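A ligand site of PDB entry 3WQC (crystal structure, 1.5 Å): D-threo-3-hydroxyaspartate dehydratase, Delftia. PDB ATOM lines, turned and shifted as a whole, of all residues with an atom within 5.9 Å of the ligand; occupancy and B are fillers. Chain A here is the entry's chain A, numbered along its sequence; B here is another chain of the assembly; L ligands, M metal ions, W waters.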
ATOM      1  N   HIS A  51     -27.389  -3.338  -8.017  1.00  0.00           N
ATOM      2  CA  HIS A  51     -26.689  -2.093  -8.125  1.00  0.00           C
ATOM      3  C   HIS A  51     -25.206  -2.382  -8.497  1.00  0.00           C
ATOM      4  O   HIS A  51     -24.456  -2.972  -7.657  1.00  0.00           O
ATOM      5  CB  HIS A  51     -26.722  -1.287  -6.824  1.00  0.00           C
ATOM      6  CG  HIS A  51     -26.537   0.181  -7.085  1.00  0.00           C
ATOM      7  ND1 HIS A  51     -25.554   0.679  -7.929  1.00  0.00           N
ATOM      8  CD2 HIS A  51     -27.301   1.302  -6.720  1.00  0.00           C
ATOM      9  CE1 HIS A  51     -25.671   1.998  -8.075  1.00  0.00           C
ATOM     10  NE2 HIS A  51     -26.734   2.404  -7.346  1.00  0.00           N
ATOM     11  N   LYS A  53     -22.778  -0.414  -8.836  1.00  0.00           N
ATOM     12  CA  LYS A  53     -21.712   0.503  -8.390  1.00  0.00           C
ATOM     13  C   LYS A  53     -20.666  -0.276  -7.546  1.00  0.00           C
ATOM     14  O   LYS A  53     -19.558   0.260  -7.403  1.00  0.00           O
ATOM     15  CB  LYS A  53     -22.263   1.664  -7.573  1.00  0.00           C
ATOM     16  CG  LYS A  53     -22.680   1.286  -6.179  1.00  0.00           C
ATOM     17  CD  LYS A  53     -23.188   2.612  -5.594  1.00  0.00           C
ATOM     18  CE  LYS A  53     -23.618   2.340  -4.222  1.00  0.00           C
ATOM     19  NZ  LYS A  53     -24.970   2.834  -3.717  1.00  0.00           N
ATOM     20  N   THR A  54     -20.996  -1.458  -7.028  1.00  0.00           N
ATOM     21  CA  THR A  54     -20.016  -2.195  -6.204  1.00  0.00           C
ATOM     22  C   THR A  54     -18.908  -2.748  -7.116  1.00  0.00           C
ATOM     23  O   THR A  54     -17.757  -2.725  -6.651  1.00  0.00           O
ATOM     24  CB  THR A  54     -20.759  -3.373  -5.512  1.00  0.00           C
ATOM     25  OG1 THR A  54     -21.655  -2.764  -4.573  1.00  0.00           O
ATOM     26  CG2 THR A  54     -19.788  -4.304  -4.748  1.00  0.00           C
ATOM     27  N   THR A  73     -29.033  -1.037 -11.632  1.00  0.00           N
ATOM     28  CA  THR A  73     -28.962   0.326 -11.121  1.00  0.00           C
ATOM     29  C   THR A  73     -27.499   0.750 -11.252  1.00  0.00           C
ATOM     30  O   THR A  73     -26.593  -0.059 -11.001  1.00  0.00           O
ATOM     31  CB  THR A  73     -29.321   0.348  -9.616  1.00  0.00           C
ATOM     32  OG1 THR A  73     -30.536  -0.417  -9.348  1.00  0.00           O
ATOM     33  CG2 THR A  73     -29.625   1.804  -9.152  1.00  0.00           C
ATOM     34  N   ALA A  94     -29.497   5.984 -10.324  1.00  0.00           N
ATOM     35  CA  ALA A  94     -30.159   6.245  -9.017  1.00  0.00           C
ATOM     36  C   ALA A  94     -29.344   7.296  -8.218  1.00  0.00           C
ATOM     37  O   ALA A  94     -29.070   7.087  -7.017  1.00  0.00           O
ATOM     38  CB  ALA A  94     -30.384   4.965  -8.239  1.00  0.00           C
ATOM     39  N   GLU A 144     -37.578  10.090  -5.931  1.00  0.00           N
ATOM     40  CA  GLU A 144     -36.883   9.476  -4.776  1.00  0.00           C
ATOM     41  C   GLU A 144     -37.542   9.903  -3.443  1.00  0.00           C
ATOM     42  O   GLU A 144     -37.822  11.100  -3.246  1.00  0.00           O
ATOM     43  CB  GLU A 144     -35.390   9.896  -4.756  1.00  0.00           C
ATOM     44  CG  GLU A 144     -34.649   9.128  -3.666  1.00  0.00           C
ATOM     45  CD  GLU A 144     -33.111   9.307  -3.738  1.00  0.00           C
ATOM     46  OE1 GLU A 144     -32.419   8.541  -3.042  1.00  0.00           O
ATOM     47  OE2 GLU A 144     -32.624  10.248  -4.389  1.00  0.00           O
ATOM     48  N   ARG A 151     -30.300  10.435   3.404  1.00  0.00           N
ATOM     49  CA  ARG A 151     -29.618  11.082   2.274  1.00  0.00           C
ATOM     50  C   ARG A 151     -30.630  11.914   1.439  1.00  0.00           C
ATOM     51  O   ARG A 151     -31.234  12.865   2.028  1.00  0.00           O
ATOM     52  CB  ARG A 151     -28.832  10.023   1.433  1.00  0.00           C
ATOM     53  CG  ARG A 151     -27.813  10.658   0.469  1.00  0.00           C
ATOM     54  CD  ARG A 151     -26.950   9.492  -0.061  1.00  0.00           C
ATOM     55  NE  ARG A 151     -27.744   8.626  -0.963  1.00  0.00           N
ATOM     56  CZ  ARG A 151     -27.331   7.398  -1.388  1.00  0.00           C
ATOM     57  NH1 ARG A 151     -26.196   6.847  -0.800  1.00  0.00           N
ATOM     58  NH2 ARG A 151     -28.027   6.705  -2.362  1.00  0.00           N
ATOM     59  N   LEU A 180     -38.806   5.459  -5.607  1.00  0.00           N
ATOM     60  CA  LEU A 180     -37.773   4.552  -5.093  1.00  0.00           C
ATOM     61  C   LEU A 180     -37.311   5.130  -3.756  1.00  0.00           C
ATOM     62  O   LEU A 180     -37.357   6.362  -3.523  1.00  0.00           O
ATOM     63  CB  LEU A 180     -36.541   4.339  -6.049  1.00  0.00           C
ATOM     64  CG  LEU A 180     -35.578   5.510  -6.128  1.00  0.00           C
ATOM     65  CD1 LEU A 180     -34.235   5.005  -6.755  1.00  0.00           C
ATOM     66  CD2 LEU A 180     -36.091   6.697  -6.938  1.00  0.00           C
ATOM     67  N   THR A 181     -36.745   4.225  -2.948  1.00  0.00           N
ATOM     68  CA  THR A 181     -36.099   4.704  -1.719  1.00  0.00           C
ATOM     69  C   THR A 181     -34.892   3.821  -1.455  1.00  0.00           C
ATOM     70  O   THR A 181     -34.920   2.636  -1.846  1.00  0.00           O
ATOM     71  CB  THR A 181     -37.101   4.714  -0.522  1.00  0.00           C
ATOM     72  OG1 THR A 181     -36.509   5.380   0.595  1.00  0.00           O
ATOM     73  CG2 THR A 181     -37.440   3.323  -0.133  1.00  0.00           C
ATOM     74  N   HIS A 182     -33.947   4.357  -0.691  1.00  0.00           N
ATOM     75  CA  HIS A 182     -32.760   3.593  -0.255  1.00  0.00           C
ATOM     76  C   HIS A 182     -32.586   3.849   1.229  1.00  0.00           C
ATOM     77  O   HIS A 182     -32.257   5.026   1.624  1.00  0.00           O
ATOM     78  CB  HIS A 182     -31.554   4.093  -1.033  1.00  0.00           C
ATOM     79  CG  HIS A 182     -30.243   3.556  -0.535  1.00  0.00           C
ATOM     80  ND1 HIS A 182     -29.897   2.225  -0.518  1.00  0.00           N
ATOM     81  CD2 HIS A 182     -29.128   4.282  -0.006  1.00  0.00           C
ATOM     82  CE1 HIS A 182     -28.575   2.119  -0.070  1.00  0.00           C
ATOM     83  NE2 HIS A 182     -28.125   3.362   0.235  1.00  0.00           N
ATOM     84  N   SER A 186     -29.549   1.723   7.291  1.00  0.00           N
ATOM     85  CA  SER A 186     -29.379   0.281   7.719  1.00  0.00           C
ATOM     86  C   SER A 186     -27.914  -0.023   8.083  1.00  0.00           C
ATOM     87  O   SER A 186     -27.682  -0.932   8.907  1.00  0.00           O
ATOM     88  CB  SER A 186     -29.916  -0.725   6.655  1.00  0.00           C
ATOM     89  OG  SER A 186     -29.013  -0.577   5.516  1.00  0.00           O
ATOM     90  N   TYR A 187     -26.965   0.739   7.556  1.00  0.00           N
ATOM     91  CA  TYR A 187     -25.565   0.411   7.815  1.00  0.00           C
ATOM     92  C   TYR A 187     -25.156   0.813   9.220  1.00  0.00           C
ATOM     93  O   TYR A 187     -24.058   0.397   9.712  1.00  0.00           O
ATOM     94  CB  TYR A 187     -24.729   1.217   6.824  1.00  0.00           C
ATOM     95  CG  TYR A 187     -24.612   0.537   5.464  1.00  0.00           C
ATOM     96  CD1 TYR A 187     -25.720   0.173   4.726  1.00  0.00           C
ATOM     97  CD2 TYR A 187     -23.299   0.248   4.958  1.00  0.00           C
ATOM     98  CE1 TYR A 187     -25.611  -0.419   3.475  1.00  0.00           C
ATOM     99  CE2 TYR A 187     -23.181  -0.369   3.716  1.00  0.00           C
ATOM    100  CZ  TYR A 187     -24.341  -0.715   2.988  1.00  0.00           C
ATOM    101  OH  TYR A 187     -24.189  -1.322   1.768  1.00  0.00           O
ATOM    102  N   GLY A 226     -34.438  -0.524  -1.355  1.00  0.00           N
ATOM    103  CA  GLY A 226     -33.363  -1.503  -1.057  1.00  0.00           C
ATOM    104  C   GLY A 226     -32.084  -0.929  -0.519  1.00  0.00           C
ATOM    105  O   GLY A 226     -31.644   0.143  -0.961  1.00  0.00           O
ATOM    106  N   SER A 227     -31.479  -1.750   0.289  1.00  0.00           N
ATOM    107  CA  SER A 227     -30.032  -1.691   0.587  1.00  0.00           C
ATOM    108  C   SER A 227     -29.758  -3.169   0.849  1.00  0.00           C
ATOM    109  O   SER A 227     -30.699  -3.948   1.078  1.00  0.00           O
ATOM    110  CB  SER A 227     -29.704  -0.824   1.826  1.00  0.00           C
ATOM    111  OG  SER A 227     -30.301  -1.412   3.001  1.00  0.00           O
ATOM    112  N   THR A 228     -28.504  -3.612   0.885  1.00  0.00           N
ATOM    113  CA  THR A 228     -28.287  -5.054   1.077  1.00  0.00           C
ATOM    114  C   THR A 228     -28.845  -5.521   2.461  1.00  0.00           C
ATOM    115  O   THR A 228     -29.480  -6.559   2.516  1.00  0.00           O
ATOM    116  CB  THR A 228     -26.733  -5.425   0.905  1.00  0.00           C
ATOM    117  OG1 THR A 228     -26.531  -5.513  -0.545  1.00  0.00           O
ATOM    118  CG2 THR A 228     -26.403  -6.752   1.547  1.00  0.00           C
ATOM    119  N   PRO A 229     -28.594  -4.775   3.549  1.00  0.00           N
ATOM    120  CA  PRO A 229     -29.071  -5.282   4.849  1.00  0.00           C
ATOM    121  C   PRO A 229     -30.625  -5.347   4.928  1.00  0.00           C
ATOM    122  O   PRO A 229     -31.178  -6.375   5.408  1.00  0.00           O
ATOM    123  CB  PRO A 229     -28.573  -4.204   5.888  1.00  0.00           C
ATOM    124  CG  PRO A 229     -27.297  -3.695   5.209  1.00  0.00           C
ATOM    125  CD  PRO A 229     -27.666  -3.639   3.686  1.00  0.00           C
ATOM    126  N   ARG A 244     -33.373  -3.184  -4.862  1.00  0.00           N
ATOM    127  CA  ARG A 244     -32.041  -2.864  -5.438  1.00  0.00           C
ATOM    128  C   ARG A 244     -31.037  -3.219  -4.356  1.00  0.00           C
ATOM    129  O   ARG A 244     -31.158  -2.765  -3.181  1.00  0.00           O
ATOM    130  CB  ARG A 244     -31.907  -1.375  -5.773  1.00  0.00           C
ATOM    131  CG  ARG A 244     -33.049  -0.862  -6.686  1.00  0.00           C
ATOM    132  CD  ARG A 244     -32.847   0.667  -6.994  1.00  0.00           C
ATOM    133  NE  ARG A 244     -32.475   1.428  -5.814  1.00  0.00           N
ATOM    134  CZ  ARG A 244     -33.302   1.655  -4.777  1.00  0.00           C
ATOM    135  NH1 ARG A 244     -34.654   1.441  -4.883  1.00  0.00           N
ATOM    136  NH2 ARG A 244     -32.791   2.159  -3.643  1.00  0.00           N
ATOM    137  N   ALA A 245     -30.018  -4.011  -4.715  1.00  0.00           N
ATOM    138  CA  ALA A 245     -28.979  -4.334  -3.712  1.00  0.00           C
ATOM    139  C   ALA A 245     -27.694  -4.509  -4.536  1.00  0.00           C
ATOM    140  O   ALA A 245     -27.782  -4.940  -5.688  1.00  0.00           O
ATOM    141  CB  ALA A 245     -29.289  -5.648  -2.975  1.00  0.00           C
ATOM    142  N   GLY A 246     -26.552  -4.153  -3.950  1.00  0.00           N
ATOM    143  CA  GLY A 246     -25.275  -4.196  -4.719  1.00  0.00           C
ATOM    144  C   GLY A 246     -24.124  -4.860  -3.991  1.00  0.00           C
ATOM    145  O   GLY A 246     -23.504  -5.795  -4.521  1.00  0.00           O
ATOM    146  N   VAL A 247     -23.888  -4.474  -2.696  1.00  0.00           N
ATOM    147  CA  VAL A 247     -22.637  -4.947  -2.107  1.00  0.00           C
ATOM    148  C   VAL A 247     -22.705  -6.433  -1.807  1.00  0.00           C
ATOM    149  O   VAL A 247     -21.644  -7.077  -1.734  1.00  0.00           O
ATOM    150  CB  VAL A 247     -22.297  -4.141  -0.807  1.00  0.00           C
ATOM    151  CG1 VAL A 247     -23.267  -4.423   0.395  1.00  0.00           C
ATOM    152  CG2 VAL A 247     -20.831  -4.403  -0.413  1.00  0.00           C
ATOM    153  N   TYR A 248     -23.912  -7.016  -1.685  1.00  0.00           N
ATOM    154  CA  TYR A 248     -24.049  -8.452  -1.376  1.00  0.00           C
ATOM    155  C   TYR A 248     -23.278  -9.331  -2.366  1.00  0.00           C
ATOM    156  O   TYR A 248     -22.984 -10.475  -2.011  1.00  0.00           O
ATOM    157  CB  TYR A 248     -25.575  -8.795  -1.433  1.00  0.00           C
ATOM    158  CG  TYR A 248     -26.053  -8.991  -2.852  1.00  0.00           C
ATOM    159  CD1 TYR A 248     -26.413  -7.880  -3.645  1.00  0.00           C
ATOM    160  CD2 TYR A 248     -26.038 -10.274  -3.472  1.00  0.00           C
ATOM    161  CE1 TYR A 248     -26.756  -8.059  -5.033  1.00  0.00           C
ATOM    162  CE2 TYR A 248     -26.368 -10.470  -4.802  1.00  0.00           C
ATOM    163  CZ  TYR A 248     -26.721  -9.357  -5.573  1.00  0.00           C
ATOM    164  OH  TYR A 248     -27.078  -9.542  -6.867  1.00  0.00           O
ATOM    165  N   MET A 255     -20.499  -5.486   6.306  1.00  0.00           N
ATOM    166  CA  MET A 255     -21.680  -6.362   6.223  1.00  0.00           C
ATOM    167  C   MET A 255     -21.647  -7.419   7.299  1.00  0.00           C
ATOM    168  O   MET A 255     -22.694  -7.742   7.907  1.00  0.00           O
ATOM    169  CB  MET A 255     -21.808  -6.998   4.844  1.00  0.00           C
ATOM    170  CG  MET A 255     -22.299  -6.000   3.767  1.00  0.00           C
ATOM    171  SD  MET A 255     -23.887  -5.179   4.108  1.00  0.00           S
ATOM    172  CE  MET A 255     -23.350  -3.485   4.270  1.00  0.00           C
ATOM    173  N   CYS A 363     -17.162  -1.958  -2.086  1.00  0.00           N
ATOM    174  CA  CYS A 363     -17.335  -0.993  -3.182  1.00  0.00           C
ATOM    175  C   CYS A 363     -16.126  -0.043  -3.211  1.00  0.00           C
ATOM    176  O   CYS A 363     -15.675   0.403  -4.287  1.00  0.00           O
ATOM    177  CB  CYS A 363     -18.568  -0.118  -2.849  1.00  0.00           C
ATOM    178  SG  CYS A 363     -20.030  -1.131  -2.326  1.00  0.00           S
ATOM    179  N   GLN B 329     -21.071   7.086  -1.734  1.00  0.00           N
ATOM    180  CA  GLN B 329     -20.183   6.838  -2.873  1.00  0.00           C
ATOM    181  C   GLN B 329     -20.197   7.970  -3.885  1.00  0.00           C
ATOM    182  O   GLN B 329     -19.139   8.496  -4.290  1.00  0.00           O
ATOM    183  CB  GLN B 329     -20.568   5.503  -3.480  1.00  0.00           C
ATOM    184  CG  GLN B 329     -19.546   5.030  -4.539  1.00  0.00           C
ATOM    185  CD  GLN B 329     -19.734   3.547  -4.892  1.00  0.00           C
ATOM    186  OE1 GLN B 329     -20.029   2.713  -3.990  1.00  0.00           O
ATOM    187  NE2 GLN B 329     -19.434   3.164  -6.151  1.00  0.00           N
ATOM    188  N   HIS B 331     -22.538  10.772  -3.523  1.00  0.00           N
ATOM    189  CA  HIS B 331     -23.268  11.917  -2.930  1.00  0.00           C
ATOM    190  C   HIS B 331     -22.412  12.440  -1.827  1.00  0.00           C
ATOM    191  O   HIS B 331     -21.950  11.666  -0.944  1.00  0.00           O
ATOM    192  CB  HIS B 331     -24.553  11.413  -2.202  1.00  0.00           C
ATOM    193  CG  HIS B 331     -25.591  10.757  -3.046  1.00  0.00           C
ATOM    194  ND1 HIS B 331     -25.492   9.507  -3.529  1.00  0.00           N
ATOM    195  CD2 HIS B 331     -26.849  11.242  -3.450  1.00  0.00           C
ATOM    196  CE1 HIS B 331     -26.614   9.183  -4.228  1.00  0.00           C
ATOM    197  NE2 HIS B 331     -27.465  10.240  -4.137  1.00  0.00           N
HETATM  198  N1  LIG L   1     -29.900   1.924  -3.980  1.00  0.00           N
HETATM  199  C1  LIG L   1     -29.204   3.089  -4.045  1.00  0.00           C
HETATM  200  C2  LIG L   1     -29.826   4.409  -4.382  1.00  0.00           C
HETATM  201  C3  LIG L   1     -27.785   3.077  -3.719  1.00  0.00           C
HETATM  202  O1  LIG L   1     -27.107   4.188  -3.811  1.00  0.00           O
HETATM  203  C4  LIG L   1     -27.170   1.825  -3.402  1.00  0.00           C
HETATM  204  C5  LIG L   1     -25.726   1.831  -3.193  1.00  0.00           C
HETATM  205  C6  LIG L   1     -28.015   0.635  -3.336  1.00  0.00           C
HETATM  206  C7  LIG L   1     -29.402   0.705  -3.634  1.00  0.00           C
HETATM  207  C8  LIG L   1     -27.413  -0.714  -3.014  1.00  0.00           C
HETATM  208  O2  LIG L   1     -27.046  -0.694  -1.566  1.00  0.00           O
HETATM  209  P1  LIG L   1     -26.123  -1.852  -0.991  1.00  0.00           P
HETATM  210  O3  LIG L   1     -26.703  -3.123  -1.512  1.00  0.00           O
HETATM  211  O4  LIG L   1     -26.278  -1.795   0.483  1.00  0.00           O
HETATM  212  O5  LIG L   1     -24.758  -1.656  -1.527  1.00  0.00           O
HETATM  213 MG    MG M   1     -21.132   0.348  -0.500  1.00  0.00          MG
HETATM  214  O   HOH W   1     -26.838   5.121  -6.860  1.00  0.00           O
HETATM  215  O   HOH W   2     -23.061   0.224  -1.219  1.00  0.00           O
HETATM  216  O   HOH W   3     -29.855   7.888  -4.320  1.00  0.00           O
HETATM  217  O   HOH W   4     -24.091  -1.293  -4.147  1.00  0.00           O
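A nitrogen (N1) of the ligand is in hydrogen-bond range of a ring nitrogen (ND1) of His 182 (3.5 Å). The guanidinium group of Arg 244 sits at hydrogen-bond distance from a nitrogen (N1) of the ligand. The side-chain hydroxyl (OG1) of Thr 228 lies within hydrogen-bond range of an oxygen (O3) of the ligand, at 2.6 Å. O4 of the ligand lies within hydrogen-bond range of N of Thr 228 (2.9 Å). The backbone NH (N) of Gly 246 lies within hydrogen-bond range of an oxygen (O3) of the ligand, at 2.7 Å. OH of Tyr 187 lies within hydrogen-bond range of O4 of the ligand (2.5 Å). NZ of Lys 53 is covalently linked to C5 of the ligand, 1.4 Å away. The guanidinium group (NH2) of Arg 151 is in hydrogen-bond range of an oxygen (O1) of the ligand (3.0 Å). The backbone NH (N) of Val 247 sits at hydrogen-bond distance from an oxygen (O5) of the ligand (3.2 Å).
The side-chain hydroxyl (OG1) of Thr 228 lies within hydrogen-bond range of the backbone NH (N) of Tyr 248 (3.2 Å). A ring nitrogen (ND1) of His 51 sits at hydrogen-bond distance from the backbone carbonyl oxygen (O) of Thr 73, 3.3 Å away. N of His 51 is in hydrogen-bond range of O of Ala 245, 2.9 Å away. The side-chain hydroxyl of Ser 227 lies within hydrogen-bond range of the side-chain hydroxyl of Ser 186 (2.9 Å). The guanidinium group (NH2) of Arg 244 lies within hydrogen-bond range of the backbone carbonyl oxygen (O) of Thr 181, at 2.8 Å. N of Val 247 lies within hydrogen-bond range of OG1 of Thr 54, at 3.4 Å. A ring nitrogen (ND1) of His 51 is in hydrogen-bond range of the backbone NH (N) of Lys 53 (3.1 Å). The backbone carbonyl oxygen (O) of Lys 53 lies within hydrogen-bond range of the side-chain amide nitrogen (NE2) of Gln 329 of chain B.
His 51 touches the ligand. Ala 94 touches the ligand (O to C2, 3.8 Å). Gly 226 touches the ligand. Ser 227 touches the ligand (CA to O4, 3.8 Å). Pro 229 touches the ligand (CD to O4, 3.9 Å). Ala 245 touches the ligand. Hydrophobic or aromatic side chains that line the ligand: His 51, Ala 94, His 182, Tyr 187, Pro 229, Ala 245 and Val 247. Within 4 Å of the ligand: His 51, Lys 53, Ala 94, Arg 151, His 182, Tyr 187, Gly 226, Ser 227, Thr 228, Pro 229, Arg 244, Ala 245, Gly 246 and Val 247. Along chain A the residues within 4 Å of the ligand span positions 51 to 247. The nearest printed residue that does not touch the ligand is Thr 54 (4.5 Å).
Water W4 bridges O5 of the ligand (2.7 Å) and OG1 of Thr 54 (2.9 Å). Water W1 lies within hydrogen-bond range of NE2 of His 51 (2.8 Å), O of Ala 94 (3.0 Å) and O1 of the ligand (3.2 Å). Water W3 lies within hydrogen-bond range of O of Ala 94 (2.9 Å), NH2 of Arg 151 (2.9 Å), OE1 of Glu 144 (2.9 Å) and NE2 of His 331 of chain B (3.4 Å).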
